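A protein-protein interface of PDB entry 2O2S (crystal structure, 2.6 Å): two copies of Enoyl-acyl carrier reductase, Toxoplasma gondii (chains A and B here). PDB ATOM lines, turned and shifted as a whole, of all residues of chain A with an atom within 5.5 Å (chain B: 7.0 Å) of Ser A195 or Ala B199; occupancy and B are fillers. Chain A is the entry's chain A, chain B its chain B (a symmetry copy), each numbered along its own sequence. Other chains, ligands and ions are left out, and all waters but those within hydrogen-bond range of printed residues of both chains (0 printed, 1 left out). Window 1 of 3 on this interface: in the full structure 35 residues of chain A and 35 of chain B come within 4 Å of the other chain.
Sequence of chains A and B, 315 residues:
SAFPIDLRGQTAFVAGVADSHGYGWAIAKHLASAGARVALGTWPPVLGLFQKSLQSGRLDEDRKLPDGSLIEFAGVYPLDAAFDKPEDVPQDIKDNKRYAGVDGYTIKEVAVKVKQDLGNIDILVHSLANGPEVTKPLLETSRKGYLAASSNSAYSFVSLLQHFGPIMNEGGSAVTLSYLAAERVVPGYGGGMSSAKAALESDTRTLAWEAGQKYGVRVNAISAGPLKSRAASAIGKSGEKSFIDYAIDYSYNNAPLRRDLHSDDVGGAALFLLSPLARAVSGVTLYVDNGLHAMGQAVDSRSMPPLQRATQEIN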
ATOM      1  N   LEU A 138     -12.832 -15.367  20.855  1.00  0.00           N
ATOM      2  CA  LEU A 138     -12.725 -16.334  21.962  1.00  0.00           C
ATOM      3  C   LEU A 138     -11.285 -16.557  22.382  1.00  0.00           C
ATOM      4  O   LEU A 138     -10.995 -16.703  23.552  1.00  0.00           O
ATOM      5  CB  LEU A 138     -13.368 -17.675  21.552  1.00  0.00           C
ATOM      6  CG  LEU A 138     -14.094 -18.498  22.632  1.00  0.00           C
ATOM      7  CD1 LEU A 138     -15.466 -17.935  22.939  1.00  0.00           C
ATOM      8  CD2 LEU A 138     -14.231 -19.957  22.203  1.00  0.00           C
ATOM      9  N   TYR A 146     -16.161 -14.060  29.949  1.00  0.00           N
ATOM     10  CA  TYR A 146     -16.899 -15.181  29.372  1.00  0.00           C
ATOM     11  C   TYR A 146     -17.926 -15.635  30.418  1.00  0.00           C
ATOM     12  O   TYR A 146     -19.089 -15.890  30.105  1.00  0.00           O
ATOM     13  CB  TYR A 146     -15.894 -16.273  29.003  1.00  0.00           C
ATOM     14  CG  TYR A 146     -16.423 -17.636  28.553  1.00  0.00           C
ATOM     15  CD1 TYR A 146     -16.224 -18.070  27.247  1.00  0.00           C
ATOM     16  CD2 TYR A 146     -17.047 -18.511  29.446  1.00  0.00           C
ATOM     17  CE1 TYR A 146     -16.656 -19.311  26.818  1.00  0.00           C
ATOM     18  CE2 TYR A 146     -17.492 -19.768  29.022  1.00  0.00           C
ATOM     19  CZ  TYR A 146     -17.296 -20.165  27.696  1.00  0.00           C
ATOM     20  OH  TYR A 146     -17.722 -21.405  27.251  1.00  0.00           O
ATOM     21  N   GLY A 192     -17.473 -14.940  24.185  1.00  0.00           N
ATOM     22  CA  GLY A 192     -18.262 -16.094  24.599  1.00  0.00           C
ATOM     23  C   GLY A 192     -19.783 -15.895  24.686  1.00  0.00           C
ATOM     24  O   GLY A 192     -20.478 -16.679  25.363  1.00  0.00           O
ATOM     25  N   MET A 193     -20.296 -14.842  24.036  1.00  0.00           N
ATOM     26  CA  MET A 193     -21.725 -14.772  23.727  1.00  0.00           C
ATOM     27  C   MET A 193     -22.154 -16.025  22.938  1.00  0.00           C
ATOM     28  O   MET A 193     -23.176 -16.617  23.250  1.00  0.00           O
ATOM     29  CB  MET A 193     -22.075 -13.549  22.869  1.00  0.00           C
ATOM     30  CG  MET A 193     -22.128 -12.180  23.560  1.00  0.00           C
ATOM     31  SD  MET A 193     -23.078 -12.195  25.075  1.00  0.00           S
ATOM     32  CE  MET A 193     -24.707 -12.664  24.532  1.00  0.00           C
ATOM     33  N   SER A 194     -21.391 -16.434  21.924  1.00  0.00           N
ATOM     34  CA  SER A 194     -21.683 -17.685  21.219  1.00  0.00           C
ATOM     35  C   SER A 194     -21.873 -18.841  22.222  1.00  0.00           C
ATOM     36  O   SER A 194     -22.877 -19.544  22.221  1.00  0.00           O
ATOM     37  CB  SER A 194     -20.615 -18.024  20.117  1.00  0.00           C
ATOM     38  OG  SER A 194     -19.259 -18.027  20.560  1.00  0.00           O
ATOM     39  N   SER A 195     -20.896 -18.989  23.102  1.00  0.00           N
ATOM     40  CA  SER A 195     -20.887 -20.023  24.099  1.00  0.00           C
ATOM     41  C   SER A 195     -22.144 -19.987  24.942  1.00  0.00           C
ATOM     42  O   SER A 195     -22.779 -21.022  25.166  1.00  0.00           O
ATOM     43  CB  SER A 195     -19.658 -19.806  24.977  1.00  0.00           C
ATOM     44  OG  SER A 195     -18.623 -19.220  24.210  1.00  0.00           O
ATOM     45  N   ALA A 196     -22.501 -18.785  25.390  1.00  0.00           N
ATOM     46  CA  ALA A 196     -23.607 -18.590  26.348  1.00  0.00           C
ATOM     47  C   ALA A 196     -24.987 -18.745  25.689  1.00  0.00           C
ATOM     48  O   ALA A 196     -25.966 -19.058  26.375  1.00  0.00           O
ATOM     49  CB  ALA A 196     -23.491 -17.230  27.013  1.00  0.00           C
ATOM     50  N   LYS A 197     -25.078 -18.497  24.376  1.00  0.00           N
ATOM     51  CA  LYS A 197     -26.322 -18.743  23.632  1.00  0.00           C
ATOM     52  C   LYS A 197     -26.529 -20.257  23.396  1.00  0.00           C
ATOM     53  O   LYS A 197     -27.643 -20.732  23.329  1.00  0.00           O
ATOM     54  CB  LYS A 197     -26.335 -17.966  22.305  1.00  0.00           C
ATOM     55  CG  LYS A 197     -26.398 -16.443  22.457  1.00  0.00           C
ATOM     56  CD  LYS A 197     -27.753 -15.977  23.027  1.00  0.00           C
ATOM     57  CE  LYS A 197     -27.800 -14.502  23.413  1.00  0.00           C
ATOM     58  NZ  LYS A 197     -29.191 -14.107  23.828  1.00  0.00           N
ATOM     59  N   ALA A 198     -25.458 -21.023  23.314  1.00  0.00           N
ATOM     60  CA  ALA A 198     -25.580 -22.465  23.132  1.00  0.00           C
ATOM     61  C   ALA A 198     -26.075 -23.051  24.461  1.00  0.00           C
ATOM     62  O   ALA A 198     -27.020 -23.828  24.512  1.00  0.00           O
ATOM     63  CB  ALA A 198     -24.246 -23.042  22.703  1.00  0.00           C
ATOM     64  N   ALA A 199     -25.464 -22.587  25.539  1.00  0.00           N
ATOM     65  CA  ALA A 199     -25.914 -22.921  26.881  1.00  0.00           C
ATOM     66  C   ALA A 199     -27.382 -22.586  27.041  1.00  0.00           C
ATOM     67  O   ALA A 199     -28.153 -23.388  27.559  1.00  0.00           O
ATOM     68  CB  ALA A 199     -25.068 -22.187  27.929  1.00  0.00           C
ATOM     69  N   LEU A 200     -27.783 -21.419  26.558  1.00  0.00           N
ATOM     70  CA  LEU A 200     -29.170 -20.958  26.693  1.00  0.00           C
ATOM     71  C   LEU A 200     -30.136 -21.889  25.964  1.00  0.00           C
ATOM     72  O   LEU A 200     -31.242 -22.206  26.469  1.00  0.00           O
ATOM     73  CB  LEU A 200     -29.298 -19.543  26.133  1.00  0.00           C
ATOM     74  CG  LEU A 200     -30.664 -18.878  26.254  1.00  0.00           C
ATOM     75  CD1 LEU A 200     -30.785 -18.157  27.549  1.00  0.00           C
ATOM     76  CD2 LEU A 200     -30.870 -17.916  25.125  1.00  0.00           C
ATOM     77  N   SER B 150     -19.327 -24.294  34.285  1.00  0.00           N
ATOM     78  CA  SER B 150     -18.934 -23.625  33.049  1.00  0.00           C
ATOM     79  C   SER B 150     -17.448 -23.331  33.088  1.00  0.00           C
ATOM     80  O   SER B 150     -16.667 -23.713  32.202  1.00  0.00           O
ATOM     81  CB  SER B 150     -19.705 -22.315  32.901  1.00  0.00           C
ATOM     82  OG  SER B 150     -19.350 -21.657  31.704  1.00  0.00           O
ATOM     83  N   ALA B 154     -15.859 -25.896  30.528  1.00  0.00           N
ATOM     84  CA  ALA B 154     -15.870 -25.239  29.203  1.00  0.00           C
ATOM     85  C   ALA B 154     -14.833 -24.110  29.010  1.00  0.00           C
ATOM     86  O   ALA B 154     -14.069 -24.142  28.027  1.00  0.00           O
ATOM     87  CB  ALA B 154     -17.241 -24.723  28.888  1.00  0.00           C
ATOM     88  N   TYR B 155     -14.774 -23.126  29.902  1.00  0.00           N
ATOM     89  CA  TYR B 155     -13.779 -22.073  29.703  1.00  0.00           C
ATOM     90  C   TYR B 155     -12.390 -22.684  29.729  1.00  0.00           C
ATOM     91  O   TYR B 155     -11.571 -22.393  28.859  1.00  0.00           O
ATOM     92  CB  TYR B 155     -13.863 -20.906  30.686  1.00  0.00           C
ATOM     93  CG  TYR B 155     -12.895 -19.800  30.276  1.00  0.00           C
ATOM     94  CD1 TYR B 155     -13.222 -18.902  29.295  1.00  0.00           C
ATOM     95  CD2 TYR B 155     -11.634 -19.697  30.836  1.00  0.00           C
ATOM     96  CE1 TYR B 155     -12.331 -17.913  28.905  1.00  0.00           C
ATOM     97  CE2 TYR B 155     -10.735 -18.708  30.453  1.00  0.00           C
ATOM     98  CZ  TYR B 155     -11.087 -17.830  29.492  1.00  0.00           C
ATOM     99  OH  TYR B 155     -10.238 -16.852  29.102  1.00  0.00           O
ATOM    100  N   VAL B 158     -11.100 -23.246  26.351  1.00  0.00           N
ATOM    101  CA  VAL B 158     -10.762 -22.050  25.623  1.00  0.00           C
ATOM    102  C   VAL B 158      -9.405 -21.561  26.128  1.00  0.00           C
ATOM    103  O   VAL B 158      -8.536 -21.183  25.345  1.00  0.00           O
ATOM    104  CB  VAL B 158     -11.880 -20.970  25.796  1.00  0.00           C
ATOM    105  CG1 VAL B 158     -11.428 -19.555  25.282  1.00  0.00           C
ATOM    106  CG2 VAL B 158     -13.181 -21.429  25.110  1.00  0.00           C
ATOM    107  N   SER B 178     -17.468 -34.230  25.295  1.00  0.00           N
ATOM    108  CA  SER B 178     -18.806 -33.860  25.706  1.00  0.00           C
ATOM    109  C   SER B 178     -19.677 -35.072  26.059  1.00  0.00           C
ATOM    110  O   SER B 178     -19.240 -36.258  26.034  1.00  0.00           O
ATOM    111  CB  SER B 178     -19.492 -33.064  24.588  1.00  0.00           C
ATOM    112  OG  SER B 178     -20.471 -32.158  25.109  1.00  0.00           O
ATOM    113  N   ALA B 182     -25.679 -32.272  26.353  1.00  0.00           N
ATOM    114  CA  ALA B 182     -25.492 -30.986  25.646  1.00  0.00           C
ATOM    115  C   ALA B 182     -26.581 -30.736  24.609  1.00  0.00           C
ATOM    116  O   ALA B 182     -27.098 -29.625  24.506  1.00  0.00           O
ATOM    117  CB  ALA B 182     -24.123 -30.959  24.990  1.00  0.00           C
ATOM    118  N   MET B 193     -24.133 -28.808  33.943  1.00  0.00           N
ATOM    119  CA  MET B 193     -23.158 -29.587  33.184  1.00  0.00           C
ATOM    120  C   MET B 193     -23.594 -29.781  31.760  1.00  0.00           C
ATOM    121  O   MET B 193     -22.776 -29.713  30.842  1.00  0.00           O
ATOM    122  CB  MET B 193     -22.994 -30.959  33.810  1.00  0.00           C
ATOM    123  CG  MET B 193     -22.241 -30.926  35.105  1.00  0.00           C
ATOM    124  SD  MET B 193     -20.486 -30.767  34.732  1.00  0.00           S
ATOM    125  CE  MET B 193     -20.118 -32.489  34.336  1.00  0.00           C
ATOM    126  N   SER B 194     -24.881 -30.079  31.581  1.00  0.00           N
ATOM    127  CA  SER B 194     -25.483 -30.122  30.268  1.00  0.00           C
ATOM    128  C   SER B 194     -25.171 -28.794  29.591  1.00  0.00           C
ATOM    129  O   SER B 194     -24.628 -28.736  28.473  1.00  0.00           O
ATOM    130  CB  SER B 194     -26.990 -30.330  30.377  1.00  0.00           C
ATOM    131  OG  SER B 194     -27.557 -29.390  31.247  1.00  0.00           O
ATOM    132  N   SER B 195     -25.455 -27.736  30.336  1.00  0.00           N
ATOM    133  CA  SER B 195     -25.322 -26.401  29.862  1.00  0.00           C
ATOM    134  C   SER B 195     -23.907 -26.173  29.380  1.00  0.00           C
ATOM    135  O   SER B 195     -23.690 -25.799  28.222  1.00  0.00           O
ATOM    136  CB  SER B 195     -25.686 -25.475  30.988  1.00  0.00           C
ATOM    137  OG  SER B 195     -26.897 -25.894  31.619  1.00  0.00           O
ATOM    138  N   ALA B 196     -22.949 -26.477  30.240  1.00  0.00           N
ATOM    139  CA  ALA B 196     -21.547 -26.284  29.939  1.00  0.00           C
ATOM    140  C   ALA B 196     -21.050 -27.072  28.742  1.00  0.00           C
ATOM    141  O   ALA B 196     -20.204 -26.573  28.003  1.00  0.00           O
ATOM    142  CB  ALA B 196     -20.710 -26.650  31.153  1.00  0.00           C
ATOM    143  N   LYS B 197     -21.540 -28.312  28.591  1.00  0.00           N
ATOM    144  CA  LYS B 197     -21.159 -29.168  27.492  1.00  0.00           C
ATOM    145  C   LYS B 197     -21.681 -28.567  26.196  1.00  0.00           C
ATOM    146  O   LYS B 197     -20.973 -28.532  25.182  1.00  0.00           O
ATOM    147  CB  LYS B 197     -21.727 -30.576  27.687  1.00  0.00           C
ATOM    148  CG  LYS B 197     -21.097 -31.445  28.811  1.00  0.00           C
ATOM    149  CD  LYS B 197     -19.564 -31.575  28.661  1.00  0.00           C
ATOM    150  CE  LYS B 197     -18.900 -32.218  29.847  1.00  0.00           C
ATOM    151  NZ  LYS B 197     -17.406 -32.240  29.687  1.00  0.00           N
ATOM    152  N   ALA B 198     -22.909 -28.054  26.221  1.00  0.00           N
ATOM    153  CA  ALA B 198     -23.439 -27.358  25.057  1.00  0.00           C
ATOM    154  C   ALA B 198     -22.482 -26.252  24.640  1.00  0.00           C
ATOM    155  O   ALA B 198     -22.190 -26.128  23.461  1.00  0.00           O
ATOM    156  CB  ALA B 198     -24.813 -26.793  25.331  1.00  0.00           C
ATOM    157  N   ALA B 199     -21.975 -25.473  25.606  1.00  0.00           N
ATOM    158  CA  ALA B 199     -20.993 -24.429  25.317  1.00  0.00           C
ATOM    159  C   ALA B 199     -19.641 -25.000  24.902  1.00  0.00           C
ATOM    160  O   ALA B 199     -18.939 -24.418  24.105  1.00  0.00           O
ATOM    161  CB  ALA B 199     -20.813 -23.495  26.511  1.00  0.00           C
ATOM    162  N   LEU B 200     -19.257 -26.123  25.468  1.00  0.00           N
ATOM    163  CA  LEU B 200     -18.042 -26.796  25.030  1.00  0.00           C
ATOM    164  C   LEU B 200     -18.166 -27.172  23.548  1.00  0.00           C
ATOM    165  O   LEU B 200     -17.186 -27.049  22.785  1.00  0.00           O
ATOM    166  CB  LEU B 200     -17.754 -28.039  25.884  1.00  0.00           C
ATOM    167  CG  LEU B 200     -16.427 -28.759  25.631  1.00  0.00           C
ATOM    168  CD1 LEU B 200     -15.249 -27.959  26.153  1.00  0.00           C
ATOM    169  CD2 LEU B 200     -16.452 -30.167  26.273  1.00  0.00           C
ATOM    170  N   GLU B 201     -19.365 -27.580  23.122  1.00  0.00           N
ATOM    171  CA  GLU B 201     -19.523 -27.957  21.726  1.00  0.00           C
ATOM    172  C   GLU B 201     -19.502 -26.737  20.851  1.00  0.00           C
ATOM    173  O   GLU B 201     -18.772 -26.719  19.860  1.00  0.00           O
ATOM    174  CB  GLU B 201     -20.748 -28.842  21.492  1.00  0.00           C
ATOM    175  CG  GLU B 201     -20.461 -30.313  21.904  1.00  0.00           C
ATOM    176  CD  GLU B 201     -21.684 -31.194  21.871  1.00  0.00           C
ATOM    177  OE1 GLU B 201     -22.470 -31.049  20.924  1.00  0.00           O
ATOM    178  OE2 GLU B 201     -21.840 -32.058  22.762  1.00  0.00           O
ATOM    179  N   SER B 202     -20.238 -25.701  21.253  1.00  0.00           N
ATOM    180  CA  SER B 202     -20.240 -24.437  20.514  1.00  0.00           C
ATOM    181  C   SER B 202     -18.820 -23.932  20.375  1.00  0.00           C
ATOM    182  O   SER B 202     -18.351 -23.687  19.277  1.00  0.00           O
ATOM    183  CB  SER B 202     -21.124 -23.361  21.166  1.00  0.00           C
ATOM    184  OG  SER B 202     -21.158 -22.159  20.369  1.00  0.00           O
ATOM    185  N   ASP B 203     -18.120 -23.835  21.492  1.00  0.00           N
ATOM    186  CA  ASP B 203     -16.731 -23.388  21.452  1.00  0.00           C
ATOM    187  C   ASP B 203     -15.779 -24.317  20.650  1.00  0.00           C
ATOM    188  O   ASP B 203     -14.829 -23.826  20.089  1.00  0.00           O
ATOM    189  CB  ASP B 203     -16.185 -23.125  22.860  1.00  0.00           C
ATOM    190  CG  ASP B 203     -16.927 -22.011  23.586  1.00  0.00           C
ATOM    191  OD1 ASP B 203     -17.816 -21.351  23.004  1.00  0.00           O
ATOM    192  OD2 ASP B 203     -16.645 -21.837  24.778  1.00  0.00           O
ATOM    193  N   THR B 204     -16.029 -25.636  20.577  1.00  0.00           N
ATOM    194  CA  THR B 204     -15.240 -26.494  19.704  1.00  0.00           C
ATOM    195  C   THR B 204     -15.355 -25.980  18.250  1.00  0.00           C
ATOM    196  O   THR B 204     -14.381 -25.996  17.496  1.00  0.00           O
ATOM    197  CB  THR B 204     -15.692 -27.955  19.814  1.00  0.00           C
ATOM    198  OG1 THR B 204     -15.465 -28.410  21.151  1.00  0.00           O
ATOM    199  CG2 THR B 204     -14.934 -28.872  18.818  1.00  0.00           C
ATOM    200  N   ARG B 205     -16.544 -25.524  17.870  1.00  0.00           N
ATOM    201  CA  ARG B 205     -16.735 -24.954  16.536  1.00  0.00           C
ATOM    202  C   ARG B 205     -16.047 -23.594  16.323  1.00  0.00           C
ATOM    203  O   ARG B 205     -15.242 -23.435  15.415  1.00  0.00           O
ATOM    204  CB  ARG B 205     -18.217 -24.869  16.189  1.00  0.00           C
ATOM    205  CG  ARG B 205     -18.844 -26.249  16.092  1.00  0.00           C
ATOM    206  CD  ARG B 205     -20.259 -26.168  15.625  1.00  0.00           C
ATOM    207  NE  ARG B 205     -21.136 -25.654  16.666  1.00  0.00           N
ATOM    208  CZ  ARG B 205     -21.718 -26.397  17.614  1.00  0.00           C
ATOM    209  NH1 ARG B 205     -21.487 -27.687  17.720  1.00  0.00           N
ATOM    210  NH2 ARG B 205     -22.533 -25.831  18.471  1.00  0.00           N
ATOM    211  N   THR B 206     -16.333 -22.642  17.184  1.00  0.00           N
ATOM    212  CA  THR B 206     -15.690 -21.340  17.149  1.00  0.00           C
ATOM    213  C   THR B 206     -14.151 -21.432  17.201  1.00  0.00           C
ATOM    214  O   THR B 206     -13.446 -20.691  16.504  1.00  0.00           O
ATOM    215  CB  THR B 206     -16.223 -20.483  18.320  1.00  0.00           C
ATOM    216  OG1 THR B 206     -17.651 -20.521  18.310  1.00  0.00           O
ATOM    217  CG2 THR B 206     -15.768 -19.058  18.228  1.00  0.00           C
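The side-chain carboxylate of Asp B203 sits at hydrogen-bond distance from the side-chain hydroxyl of Ser A195. OD2 of Asp B203 sits at hydrogen-bond distance from OH of Tyr A146 (2.7 Å).
The backbone carbonyl oxygen of Gly A192 lies close to the side-chain hydroxyl of Ser A195 (3.4 Å). O of Ser B202 sits at hydrogen-bond distance from OG1 of Thr B206 (3.4 Å). O of Ser B150 is in hydrogen-bond range of N of Tyr B155.
O of Leu A138 touches CG1 of Val B158 (3.4 Å). OG of Ser B150 touches CE2 of Tyr A146 (3.8 Å). OH of Tyr A146 touches CB of Ala B154, at 3.7 Å. Tyr A146 touches Tyr B155 (CG to CD1, 3.5 Å). Tyr A146 touches Ala B199 (OH to CB, 3.8 Å). Thr B206 touches Ser A194. Ser A195 touches Ala B199. Ala B198 touches Ala A198. Ser B202 touches Ala A198 (CB to CB, 3.5 Å). CA of Ala A199 touches O of Ser B195, at 3.9 Å.
Of chain B, only Ala B199 and Asp B203 come within 4 Å of Ser A195. Of the printed residues of chain A, Ser B195 touches Ala A199 (3.9 Å). Printed residues of chain A within 4 Å of Asp B203: Leu A138 (3.7 Å), Tyr A146 (2.7 Å) and Ser A195 (2.6 Å). Of the printed residues of chain B, Ser A194 touches Ser B202 (3.6 Å) and Thr B206 (3.7 Å). Of the printed residues of chain A, Ala B198 touches Ala A198 (3.8 Å). Ala A196 touches none of the printed residues of chain B. Glu B201 touches none of the printed residues of chain A. The nearest residue of chain B that does not touch Ser A195 is Ser B202 (4.2 Å).
Of the 20 printed residues of chain B, 10 touch a printed residue of chain A. Hydrophobic or aromatic side chains of chain B within 4 Å of the printed part of chain A: Ala B154, Tyr B155, Val B158, Ala B198 and Ala B199. Hydrophobic or aromatic side chains of chain A within 4 Å of the printed part of chain B: Leu A138, Tyr A146, Ala A198 and Ala A199. Among the printed residues, 14 pairs touch across the chains.
Ser A195 touches Ala B199, and with the chains exchanged Ala A199 touches Ser B195. Ala A198 touches its own counterpart, Ala B198. Of the 14 pairs that touch across the chains among the printed residues, 3 have their exchanged pair printed and touching as well.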
